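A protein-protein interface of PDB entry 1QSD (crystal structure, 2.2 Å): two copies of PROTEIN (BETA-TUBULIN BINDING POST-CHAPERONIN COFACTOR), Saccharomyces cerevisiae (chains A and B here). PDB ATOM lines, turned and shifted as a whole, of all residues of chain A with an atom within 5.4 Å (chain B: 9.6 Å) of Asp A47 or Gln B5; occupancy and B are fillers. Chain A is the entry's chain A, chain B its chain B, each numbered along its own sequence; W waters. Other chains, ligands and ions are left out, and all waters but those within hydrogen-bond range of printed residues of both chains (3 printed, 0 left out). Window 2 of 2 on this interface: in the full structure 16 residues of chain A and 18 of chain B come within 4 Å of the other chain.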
ATOM      1  N   LEU A  37      25.143 -29.594 -18.419  1.00  0.00           N
ATOM      2  CA  LEU A  37      23.745 -29.282 -18.111  1.00  0.00           C
ATOM      3  C   LEU A  37      23.032 -28.598 -19.280  1.00  0.00           C
ATOM      4  O   LEU A  37      21.806 -28.674 -19.406  1.00  0.00           O
ATOM      5  CB  LEU A  37      23.641 -28.361 -16.905  1.00  0.00           C
ATOM      6  CG  LEU A  37      24.096 -28.932 -15.584  1.00  0.00           C
ATOM      7  CD1 LEU A  37      23.889 -27.905 -14.499  1.00  0.00           C
ATOM      8  CD2 LEU A  37      23.312 -30.173 -15.308  1.00  0.00           C
ATOM      9  N   VAL A  43      16.977 -30.945 -18.382  1.00  0.00           N
ATOM     10  CA  VAL A  43      17.294 -30.094 -17.228  1.00  0.00           C
ATOM     11  C   VAL A  43      16.460 -28.821 -17.079  1.00  0.00           C
ATOM     12  O   VAL A  43      16.273 -28.022 -17.999  1.00  0.00           O
ATOM     13  CB  VAL A  43      18.805 -29.764 -17.143  1.00  0.00           C
ATOM     14  CG1 VAL A  43      19.082 -28.790 -16.032  1.00  0.00           C
ATOM     15  CG2 VAL A  43      19.604 -31.044 -16.926  1.00  0.00           C
ATOM     16  N   ASP A  44      15.978 -28.644 -15.855  1.00  0.00           N
ATOM     17  CA  ASP A  44      15.148 -27.514 -15.466  1.00  0.00           C
ATOM     18  C   ASP A  44      15.911 -26.195 -15.626  1.00  0.00           C
ATOM     19  O   ASP A  44      16.990 -26.027 -15.070  1.00  0.00           O
ATOM     20  CB  ASP A  44      14.716 -27.701 -14.017  1.00  0.00           C
ATOM     21  CG  ASP A  44      13.879 -26.543 -13.506  1.00  0.00           C
ATOM     22  OD1 ASP A  44      14.399 -25.726 -12.726  1.00  0.00           O
ATOM     23  OD2 ASP A  44      12.703 -26.432 -13.904  1.00  0.00           O
ATOM     24  N   PRO A  45      15.336 -25.227 -16.342  1.00  0.00           N
ATOM     25  CA  PRO A  45      15.983 -23.922 -16.560  1.00  0.00           C
ATOM     26  C   PRO A  45      16.626 -23.261 -15.318  1.00  0.00           C
ATOM     27  O   PRO A  45      17.705 -22.668 -15.391  1.00  0.00           O
ATOM     28  CB  PRO A  45      14.858 -23.067 -17.164  1.00  0.00           C
ATOM     29  CG  PRO A  45      13.623 -23.921 -17.116  1.00  0.00           C
ATOM     30  CD  PRO A  45      14.105 -25.334 -17.130  1.00  0.00           C
ATOM     31  N   TYR A  46      15.986 -23.428 -14.177  1.00  0.00           N
ATOM     32  CA  TYR A  46      16.490 -22.879 -12.946  1.00  0.00           C
ATOM     33  C   TYR A  46      17.780 -23.587 -12.478  1.00  0.00           C
ATOM     34  O   TYR A  46      18.708 -22.941 -12.020  1.00  0.00           O
ATOM     35  CB  TYR A  46      15.392 -22.921 -11.875  1.00  0.00           C
ATOM     36  CG  TYR A  46      15.833 -22.370 -10.546  1.00  0.00           C
ATOM     37  CD1 TYR A  46      16.260 -21.043 -10.429  1.00  0.00           C
ATOM     38  CD2 TYR A  46      15.924 -23.203  -9.423  1.00  0.00           C
ATOM     39  CE1 TYR A  46      16.777 -20.562  -9.232  1.00  0.00           C
ATOM     40  CE2 TYR A  46      16.433 -22.739  -8.231  1.00  0.00           C
ATOM     41  CZ  TYR A  46      16.860 -21.428  -8.137  1.00  0.00           C
ATOM     42  OH  TYR A  46      17.370 -20.995  -6.944  1.00  0.00           O
ATOM     43  N   ASP A  47      17.885 -24.892 -12.635  1.00  0.00           N
ATOM     44  CA  ASP A  47      19.116 -25.551 -12.201  1.00  0.00           C
ATOM     45  C   ASP A  47      20.280 -25.144 -13.087  1.00  0.00           C
ATOM     46  O   ASP A  47      21.410 -25.005 -12.617  1.00  0.00           O
ATOM     47  CB  ASP A  47      18.974 -27.067 -12.204  1.00  0.00           C
ATOM     48  CG  ASP A  47      18.027 -27.560 -11.131  1.00  0.00           C
ATOM     49  OD1 ASP A  47      17.211 -28.477 -11.412  1.00  0.00           O
ATOM     50  OD2 ASP A  47      18.096 -27.033 -10.007  1.00  0.00           O
ATOM     51  N   LEU A  48      20.016 -25.000 -14.382  1.00  0.00           N
ATOM     52  CA  LEU A  48      21.067 -24.586 -15.302  1.00  0.00           C
ATOM     53  C   LEU A  48      21.480 -23.152 -14.917  1.00  0.00           C
ATOM     54  O   LEU A  48      22.661 -22.842 -14.777  1.00  0.00           O
ATOM     55  CB  LEU A  48      20.553 -24.636 -16.754  1.00  0.00           C
ATOM     56  CG  LEU A  48      21.364 -23.899 -17.817  1.00  0.00           C
ATOM     57  CD1 LEU A  48      22.732 -24.518 -17.998  1.00  0.00           C
ATOM     58  CD2 LEU A  48      20.585 -23.919 -19.112  1.00  0.00           C
ATOM     59  N   LYS A  49      20.487 -22.301 -14.703  1.00  0.00           N
ATOM     60  CA  LYS A  49      20.718 -20.901 -14.358  1.00  0.00           C
ATOM     61  C   LYS A  49      21.565 -20.729 -13.073  1.00  0.00           C
ATOM     62  O   LYS A  49      22.468 -19.891 -13.026  1.00  0.00           O
ATOM     63  CB  LYS A  49      19.377 -20.183 -14.263  1.00  0.00           C
ATOM     64  CG  LYS A  49      19.454 -18.708 -14.214  1.00  0.00           C
ATOM     65  CD  LYS A  49      20.061 -18.130 -15.455  1.00  0.00           C
ATOM     66  CE  LYS A  49      21.584 -18.078 -15.392  1.00  0.00           C
ATOM     67  NZ  LYS A  49      22.173 -17.534 -16.648  1.00  0.00           N
ATOM     68  N   LYS A  50      21.317 -21.561 -12.060  1.00  0.00           N
ATOM     69  CA  LYS A  50      22.099 -21.507 -10.818  1.00  0.00           C
ATOM     70  C   LYS A  50      23.583 -21.633 -11.156  1.00  0.00           C
ATOM     71  O   LYS A  50      24.406 -20.850 -10.702  1.00  0.00           O
ATOM     72  CB  LYS A  50      21.682 -22.638  -9.875  1.00  0.00           C
ATOM     73  CG  LYS A  50      20.370 -22.382  -9.177  1.00  0.00           C
ATOM     74  CD  LYS A  50      19.808 -23.650  -8.511  1.00  0.00           C
ATOM     75  CE  LYS A  50      20.722 -24.163  -7.425  1.00  0.00           C
ATOM     76  NZ  LYS A  50      20.118 -25.274  -6.685  1.00  0.00           N
ATOM     77  N   GLN A  51      23.889 -22.567 -12.039  1.00  0.00           N
ATOM     78  CA  GLN A  51      25.246 -22.832 -12.459  1.00  0.00           C
ATOM     79  C   GLN A  51      25.845 -21.777 -13.355  1.00  0.00           C
ATOM     80  O   GLN A  51      27.034 -21.502 -13.265  1.00  0.00           O
ATOM     81  CB  GLN A  51      25.318 -24.173 -13.167  1.00  0.00           C
ATOM     82  CG  GLN A  51      26.428 -25.040 -12.660  1.00  0.00           C
ATOM     83  CD  GLN A  51      26.074 -25.706 -11.349  1.00  0.00           C
ATOM     84  OE1 GLN A  51      26.198 -26.929 -11.209  1.00  0.00           O
ATOM     85  NE2 GLN A  51      25.629 -24.917 -10.378  1.00  0.00           N
ATOM     86  N   THR B   4      19.150 -37.108 -12.191  1.00  0.00           N
ATOM     87  CA  THR B   4      17.874 -36.749 -11.476  1.00  0.00           C
ATOM     88  C   THR B   4      17.985 -35.322 -10.930  1.00  0.00           C
ATOM     89  O   THR B   4      19.092 -34.846 -10.657  1.00  0.00           O
ATOM     90  CB  THR B   4      17.589 -37.722 -10.308  1.00  0.00           C
ATOM     91  OG1 THR B   4      18.580 -37.554  -9.282  1.00  0.00           O
ATOM     92  CG2 THR B   4      17.684 -39.163 -10.794  1.00  0.00           C
ATOM     93  N   GLN B   5      16.851 -34.642 -10.782  1.00  0.00           N
ATOM     94  CA  GLN B   5      16.847 -33.270 -10.274  1.00  0.00           C
ATOM     95  C   GLN B   5      17.497 -33.199  -8.880  1.00  0.00           C
ATOM     96  O   GLN B   5      18.294 -32.301  -8.628  1.00  0.00           O
ATOM     97  CB  GLN B   5      15.431 -32.699 -10.266  1.00  0.00           C
ATOM     98  CG  GLN B   5      15.418 -31.199 -10.145  1.00  0.00           C
ATOM     99  CD  GLN B   5      14.052 -30.584 -10.293  1.00  0.00           C
ATOM    100  OE1 GLN B   5      13.926 -29.358 -10.422  1.00  0.00           O
ATOM    101  NE2 GLN B   5      13.012 -31.408 -10.255  1.00  0.00           N
ATOM    102  N   LEU B   6      17.225 -34.194  -8.028  1.00  0.00           N
ATOM    103  CA  LEU B   6      17.809 -34.281  -6.669  1.00  0.00           C
ATOM    104  C   LEU B   6      19.323 -34.232  -6.752  1.00  0.00           C
ATOM    105  O   LEU B   6      19.977 -33.386  -6.108  1.00  0.00           O
ATOM    106  CB  LEU B   6      17.419 -35.593  -5.980  1.00  0.00           C
ATOM    107  CG  LEU B   6      18.037 -35.825  -4.586  1.00  0.00           C
ATOM    108  CD1 LEU B   6      17.560 -34.716  -3.652  1.00  0.00           C
ATOM    109  CD2 LEU B   6      17.633 -37.199  -4.024  1.00  0.00           C
ATOM    110  N   ASP B   7      19.862 -35.134  -7.575  1.00  0.00           N
ATOM    111  CA  ASP B   7      21.297 -35.234  -7.803  1.00  0.00           C
ATOM    112  C   ASP B   7      21.922 -33.915  -8.274  1.00  0.00           C
ATOM    113  O   ASP B   7      23.011 -33.538  -7.821  1.00  0.00           O
ATOM    114  CB  ASP B   7      21.586 -36.359  -8.801  1.00  0.00           C
ATOM    115  CG  ASP B   7      21.269 -37.746  -8.237  1.00  0.00           C
ATOM    116  OD1 ASP B   7      21.189 -38.705  -9.037  1.00  0.00           O
ATOM    117  OD2 ASP B   7      21.094 -37.893  -6.996  1.00  0.00           O
ATOM    118  N   ILE B   8      21.216 -33.200  -9.149  1.00  0.00           N
ATOM    119  CA  ILE B   8      21.715 -31.937  -9.668  1.00  0.00           C
ATOM    120  C   ILE B   8      21.761 -30.907  -8.536  1.00  0.00           C
ATOM    121  O   ILE B   8      22.774 -30.216  -8.361  1.00  0.00           O
ATOM    122  CB  ILE B   8      20.844 -31.434 -10.885  1.00  0.00           C
ATOM    123  CG1 ILE B   8      21.036 -32.364 -12.092  1.00  0.00           C
ATOM    124  CG2 ILE B   8      21.262 -30.031 -11.345  1.00  0.00           C
ATOM    125  CD1 ILE B   8      20.107 -32.025 -13.251  1.00  0.00           C
ATOM    126  N   LYS B   9      20.687 -30.815  -7.754  1.00  0.00           N
ATOM    127  CA  LYS B   9      20.635 -29.850  -6.647  1.00  0.00           C
ATOM    128  C   LYS B   9      21.661 -30.163  -5.562  1.00  0.00           C
ATOM    129  O   LYS B   9      22.246 -29.261  -5.010  1.00  0.00           O
ATOM    130  CB  LYS B   9      19.231 -29.773  -6.046  1.00  0.00           C
ATOM    131  CG  LYS B   9      18.219 -29.117  -6.966  1.00  0.00           C
ATOM    132  CD  LYS B   9      16.904 -28.890  -6.278  1.00  0.00           C
ATOM    133  CE  LYS B   9      15.859 -28.419  -7.280  1.00  0.00           C
ATOM    134  NZ  LYS B   9      16.238 -27.150  -7.929  1.00  0.00           N
ATOM    135  N   VAL B  10      21.912 -31.440  -5.296  1.00  0.00           N
ATOM    136  CA  VAL B  10      22.911 -31.812  -4.297  1.00  0.00           C
ATOM    137  C   VAL B  10      24.302 -31.448  -4.778  1.00  0.00           C
ATOM    138  O   VAL B  10      25.075 -30.864  -4.022  1.00  0.00           O
ATOM    139  CB  VAL B  10      22.916 -33.322  -3.993  1.00  0.00           C
ATOM    140  CG1 VAL B  10      24.067 -33.648  -3.047  1.00  0.00           C
ATOM    141  CG2 VAL B  10      21.577 -33.761  -3.386  1.00  0.00           C
ATOM    142  N   LYS B  11      24.652 -31.835  -6.009  1.00  0.00           N
ATOM    143  CA  LYS B  11      25.978 -31.508  -6.557  1.00  0.00           C
ATOM    144  C   LYS B  11      26.200 -30.008  -6.690  1.00  0.00           C
ATOM    145  O   LYS B  11      27.314 -29.532  -6.505  1.00  0.00           O
ATOM    146  CB  LYS B  11      26.223 -32.189  -7.904  1.00  0.00           C
ATOM    147  CG  LYS B  11      26.417 -33.689  -7.786  1.00  0.00           C
ATOM    148  CD  LYS B  11      26.430 -34.388  -9.146  1.00  0.00           C
ATOM    149  CE  LYS B  11      26.669 -35.904  -8.972  1.00  0.00           C
ATOM    150  NZ  LYS B  11      26.584 -36.724 -10.238  1.00  0.00           N
ATOM    151  N   ALA B  12      25.152 -29.254  -6.999  1.00  0.00           N
ATOM    152  CA  ALA B  12      25.306 -27.821  -7.123  1.00  0.00           C
ATOM    153  C   ALA B  12      25.802 -27.269  -5.791  1.00  0.00           C
ATOM    154  O   ALA B  12      26.749 -26.499  -5.765  1.00  0.00           O
ATOM    155  CB  ALA B  12      24.008 -27.184  -7.501  1.00  0.00           C
ATOM    156  N   LEU B  13      25.203 -27.707  -4.684  1.00  0.00           N
ATOM    157  CA  LEU B  13      25.593 -27.240  -3.355  1.00  0.00           C
ATOM    158  C   LEU B  13      26.926 -27.787  -2.925  1.00  0.00           C
ATOM    159  O   LEU B  13      27.753 -27.042  -2.433  1.00  0.00           O
ATOM    160  CB  LEU B  13      24.542 -27.603  -2.302  1.00  0.00           C
ATOM    161  CG  LEU B  13      24.695 -27.079  -0.851  1.00  0.00           C
ATOM    162  CD1 LEU B  13      24.687 -25.536  -0.832  1.00  0.00           C
ATOM    163  CD2 LEU B  13      23.566 -27.640   0.048  1.00  0.00           C
ATOM    164  N   GLU B  71      21.272 -19.591  -0.922  1.00  0.00           N
ATOM    165  CA  GLU B  71      20.230 -19.843  -1.937  1.00  0.00           C
ATOM    166  C   GLU B  71      20.214 -21.307  -2.298  1.00  0.00           C
ATOM    167  O   GLU B  71      19.160 -21.937  -2.323  1.00  0.00           O
ATOM    168  CB  GLU B  71      20.504 -19.109  -3.252  1.00  0.00           C
ATOM    169  CG  GLU B  71      20.459 -17.600  -3.203  1.00  0.00           C
ATOM    170  CD  GLU B  71      21.122 -16.969  -4.437  1.00  0.00           C
ATOM    171  OE1 GLU B  71      21.538 -15.779  -4.359  1.00  0.00           O
ATOM    172  OE2 GLU B  71      21.253 -17.681  -5.471  1.00  0.00           O
ATOM    173  N   PHE B  72      21.391 -21.829  -2.616  1.00  0.00           N
ATOM    174  CA  PHE B  72      21.535 -23.217  -3.016  1.00  0.00           C
ATOM    175  C   PHE B  72      21.047 -24.159  -1.922  1.00  0.00           C
ATOM    176  O   PHE B  72      20.360 -25.158  -2.207  1.00  0.00           O
ATOM    177  CB  PHE B  72      22.986 -23.534  -3.428  1.00  0.00           C
ATOM    178  CG  PHE B  72      23.379 -22.980  -4.802  1.00  0.00           C
ATOM    179  CD1 PHE B  72      22.880 -21.768  -5.261  1.00  0.00           C
ATOM    180  CD2 PHE B  72      24.283 -23.672  -5.619  1.00  0.00           C
ATOM    181  CE1 PHE B  72      23.263 -21.250  -6.511  1.00  0.00           C
ATOM    182  CE2 PHE B  72      24.670 -23.158  -6.867  1.00  0.00           C
ATOM    183  CZ  PHE B  72      24.160 -21.945  -7.307  1.00  0.00           C
ATOM    184  N   ASP B  75      17.251 -23.878  -1.611  1.00  0.00           N
ATOM    185  CA  ASP B  75      16.653 -24.511  -2.759  1.00  0.00           C
ATOM    186  C   ASP B  75      16.565 -26.005  -2.468  1.00  0.00           C
ATOM    187  O   ASP B  75      15.506 -26.611  -2.606  1.00  0.00           O
ATOM    188  CB  ASP B  75      17.505 -24.263  -4.013  1.00  0.00           C
ATOM    189  CG  ASP B  75      16.880 -24.860  -5.259  1.00  0.00           C
ATOM    190  OD1 ASP B  75      17.624 -25.485  -6.056  1.00  0.00           O
ATOM    191  OD2 ASP B  75      15.637 -24.722  -5.423  1.00  0.00           O
ATOM    192  N   LEU B  76      17.677 -26.587  -2.049  1.00  0.00           N
ATOM    193  CA  LEU B  76      17.714 -28.012  -1.743  1.00  0.00           C
ATOM    194  C   LEU B  76      16.768 -28.372  -0.598  1.00  0.00           C
ATOM    195  O   LEU B  76      16.052 -29.359  -0.698  1.00  0.00           O
ATOM    196  CB  LEU B  76      19.149 -28.488  -1.462  1.00  0.00           C
ATOM    197  CG  LEU B  76      19.391 -29.995  -1.272  1.00  0.00           C
ATOM    198  CD1 LEU B  76      18.795 -30.790  -2.410  1.00  0.00           C
ATOM    199  CD2 LEU B  76      20.893 -30.300  -1.177  1.00  0.00           C
ATOM    200  N   PHE B  79      13.168 -28.304  -1.872  1.00  0.00           N
ATOM    201  CA  PHE B  79      12.939 -29.446  -2.742  1.00  0.00           C
ATOM    202  C   PHE B  79      12.691 -30.709  -1.911  1.00  0.00           C
ATOM    203  O   PHE B  79      11.881 -31.536  -2.272  1.00  0.00           O
ATOM    204  CB  PHE B  79      14.146 -29.644  -3.664  1.00  0.00           C
ATOM    205  CG  PHE B  79      14.041 -30.844  -4.564  1.00  0.00           C
ATOM    206  CD1 PHE B  79      13.341 -30.772  -5.771  1.00  0.00           C
ATOM    207  CD2 PHE B  79      14.663 -32.036  -4.232  1.00  0.00           C
ATOM    208  CE1 PHE B  79      13.278 -31.875  -6.627  1.00  0.00           C
ATOM    209  CE2 PHE B  79      14.604 -33.137  -5.080  1.00  0.00           C
ATOM    210  CZ  PHE B  79      13.913 -33.058  -6.275  1.00  0.00           C
ATOM    211  N   LEU B  80      13.422 -30.873  -0.819  1.00  0.00           N
ATOM    212  CA  LEU B  80      13.255 -32.051   0.020  1.00  0.00           C
ATOM    213  C   LEU B  80      11.944 -32.117   0.822  1.00  0.00           C
ATOM    214  O   LEU B  80      11.505 -33.203   1.179  1.00  0.00           O
ATOM    215  CB  LEU B  80      14.443 -32.204   0.965  1.00  0.00           C
ATOM    216  CG  LEU B  80      15.798 -32.662   0.410  1.00  0.00           C
ATOM    217  CD1 LEU B  80      16.863 -32.412   1.467  1.00  0.00           C
ATOM    218  CD2 LEU B  80      15.773 -34.155   0.007  1.00  0.00           C
ATOM    219  N   THR B  82       8.983 -31.653  -0.201  1.00  0.00           N
ATOM    220  CA  THR B  82       7.947 -32.244  -1.042  1.00  0.00           C
ATOM    221  C   THR B  82       8.438 -33.414  -1.900  1.00  0.00           C
ATOM    222  O   THR B  82       7.742 -33.883  -2.805  1.00  0.00           O
ATOM    223  CB  THR B  82       7.323 -31.182  -1.951  1.00  0.00           C
ATOM    224  OG1 THR B  82       8.363 -30.477  -2.629  1.00  0.00           O
ATOM    225  CG2 THR B  82       6.506 -30.182  -1.138  1.00  0.00           C
ATOM    226  N   TYR B  83       9.601 -33.948  -1.558  1.00  0.00           N
ATOM    227  CA  TYR B  83      10.171 -35.049  -2.315  1.00  0.00           C
ATOM    228  C   TYR B  83       9.537 -36.388  -2.017  1.00  0.00           C
ATOM    229  O   TYR B  83       9.642 -36.900  -0.898  1.00  0.00           O
ATOM    230  CB  TYR B  83      11.658 -35.142  -2.064  1.00  0.00           C
ATOM    231  CG  TYR B  83      12.348 -36.218  -2.861  1.00  0.00           C
ATOM    232  CD1 TYR B  83      12.581 -36.058  -4.224  1.00  0.00           C
ATOM    233  CD2 TYR B  83      12.809 -37.377  -2.236  1.00  0.00           C
ATOM    234  CE1 TYR B  83      13.262 -37.034  -4.952  1.00  0.00           C
ATOM    235  CE2 TYR B  83      13.485 -38.348  -2.943  1.00  0.00           C
ATOM    236  CZ  TYR B  83      13.712 -38.172  -4.305  1.00  0.00           C
ATOM    237  OH  TYR B  83      14.384 -39.153  -4.988  1.00  0.00           O
ATOM    238  N   GLU B  87      14.860 -42.118  -4.110  1.00  0.00           N
ATOM    239  CA  GLU B  87      16.295 -42.025  -3.830  1.00  0.00           C
ATOM    240  C   GLU B  87      16.569 -41.821  -2.357  1.00  0.00           C
ATOM    241  O   GLU B  87      15.725 -41.297  -1.628  1.00  0.00           O
ATOM    242  CB  GLU B  87      16.967 -40.887  -4.589  1.00  0.00           C
ATOM    243  CG  GLU B  87      17.102 -41.096  -6.056  1.00  0.00           C
ATOM    244  CD  GLU B  87      17.929 -40.002  -6.709  1.00  0.00           C
ATOM    245  OE1 GLU B  87      17.344 -39.084  -7.319  1.00  0.00           O
ATOM    246  OE2 GLU B  87      19.169 -40.046  -6.596  1.00  0.00           O
ATOM    247  N   ALA B  92      21.929 -35.561   0.462  1.00  0.00           N
ATOM    248  CA  ALA B  92      21.322 -34.237   0.399  1.00  0.00           C
ATOM    249  C   ALA B  92      21.294 -33.594   1.788  1.00  0.00           C
ATOM    250  O   ALA B  92      21.644 -32.441   1.928  1.00  0.00           O
ATOM    251  CB  ALA B  92      19.918 -34.313  -0.178  1.00  0.00           C
HETATM  252  O   HOH W   1      24.494 -29.596 -10.525  1.00  0.00           O
HETATM  253  O   HOH W   2      21.295 -26.594  -4.673  1.00  0.00           O
HETATM  254  O   HOH W   3      18.895 -18.654  -6.019  1.00  0.00           O
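Ile B8 touches Val A43 (CD1 to CG2, 3.8 Å). Asp B75 touches Tyr A46. CG of Gln B5 touches OD1 of Asp A47, 3.5 Å away. Asp A47 touches Ile B8 (CB to CG2, 3.8 Å). Lys A50 touches Phe B72.
No position is printed for both chains. Of the 7 pairs that touch across the chains among the printed residues, none has its exchanged pair printed and touching as well.
Hydrophobic or aromatic side chains of chain A within 4 Å of the printed part of chain B: Val A43 and Tyr A46. Among the printed residues, Asp or Glu carboxylates within 4 Å of a Lys or Arg side-chain nitrogen of the other chain: Asp A47 with Lys B9 and Lys A50 with Asp B75.
Water W3 bridges OE2 of Glu B71 (2.6 Å) and OH of Tyr A46 (2.9 Å). Water W2 lies within hydrogen-bond range of NZ of Lys A50 (2.7 Å), O of Lys B9 (2.9 Å) and O of Phe B72 (3.0 Å). Water W1 bridges the backbone carbonyl oxygen of Ile B8 and the side-chain amide oxygen of Gln A51.
Of the printed residues of chain B, Asp A47 touches Gln B5, Ile B8 and Lys B9. Of chain B, only Phe B72 (3.6 Å) and Asp B75 (2.6 Å) come within 4 Å of Lys A50. Printed residues of chain A within 4 Å of Lys B9: Asp A47. Printed residues of chain B within 4 Å of Tyr A46: Asp B75. Thr B82 touches none of the printed residues of chain A.
OD1 of Asp A44 sits close to N of Tyr A46 (3.1 Å). The side-chain amino group (NZ) of Lys B9 lies within salt-bridge range of the side-chain carboxylate (OD1) of Asp B75 (2.9 Å).
OD1 of Asp B75 is in salt-bridge range of NZ of Lys A50 (2.6 Å). The side-chain carboxylate (OD2) of Asp A47 lies within salt-bridge range of the side-chain amino group (NZ) of Lys B9, 2.8 Å away.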
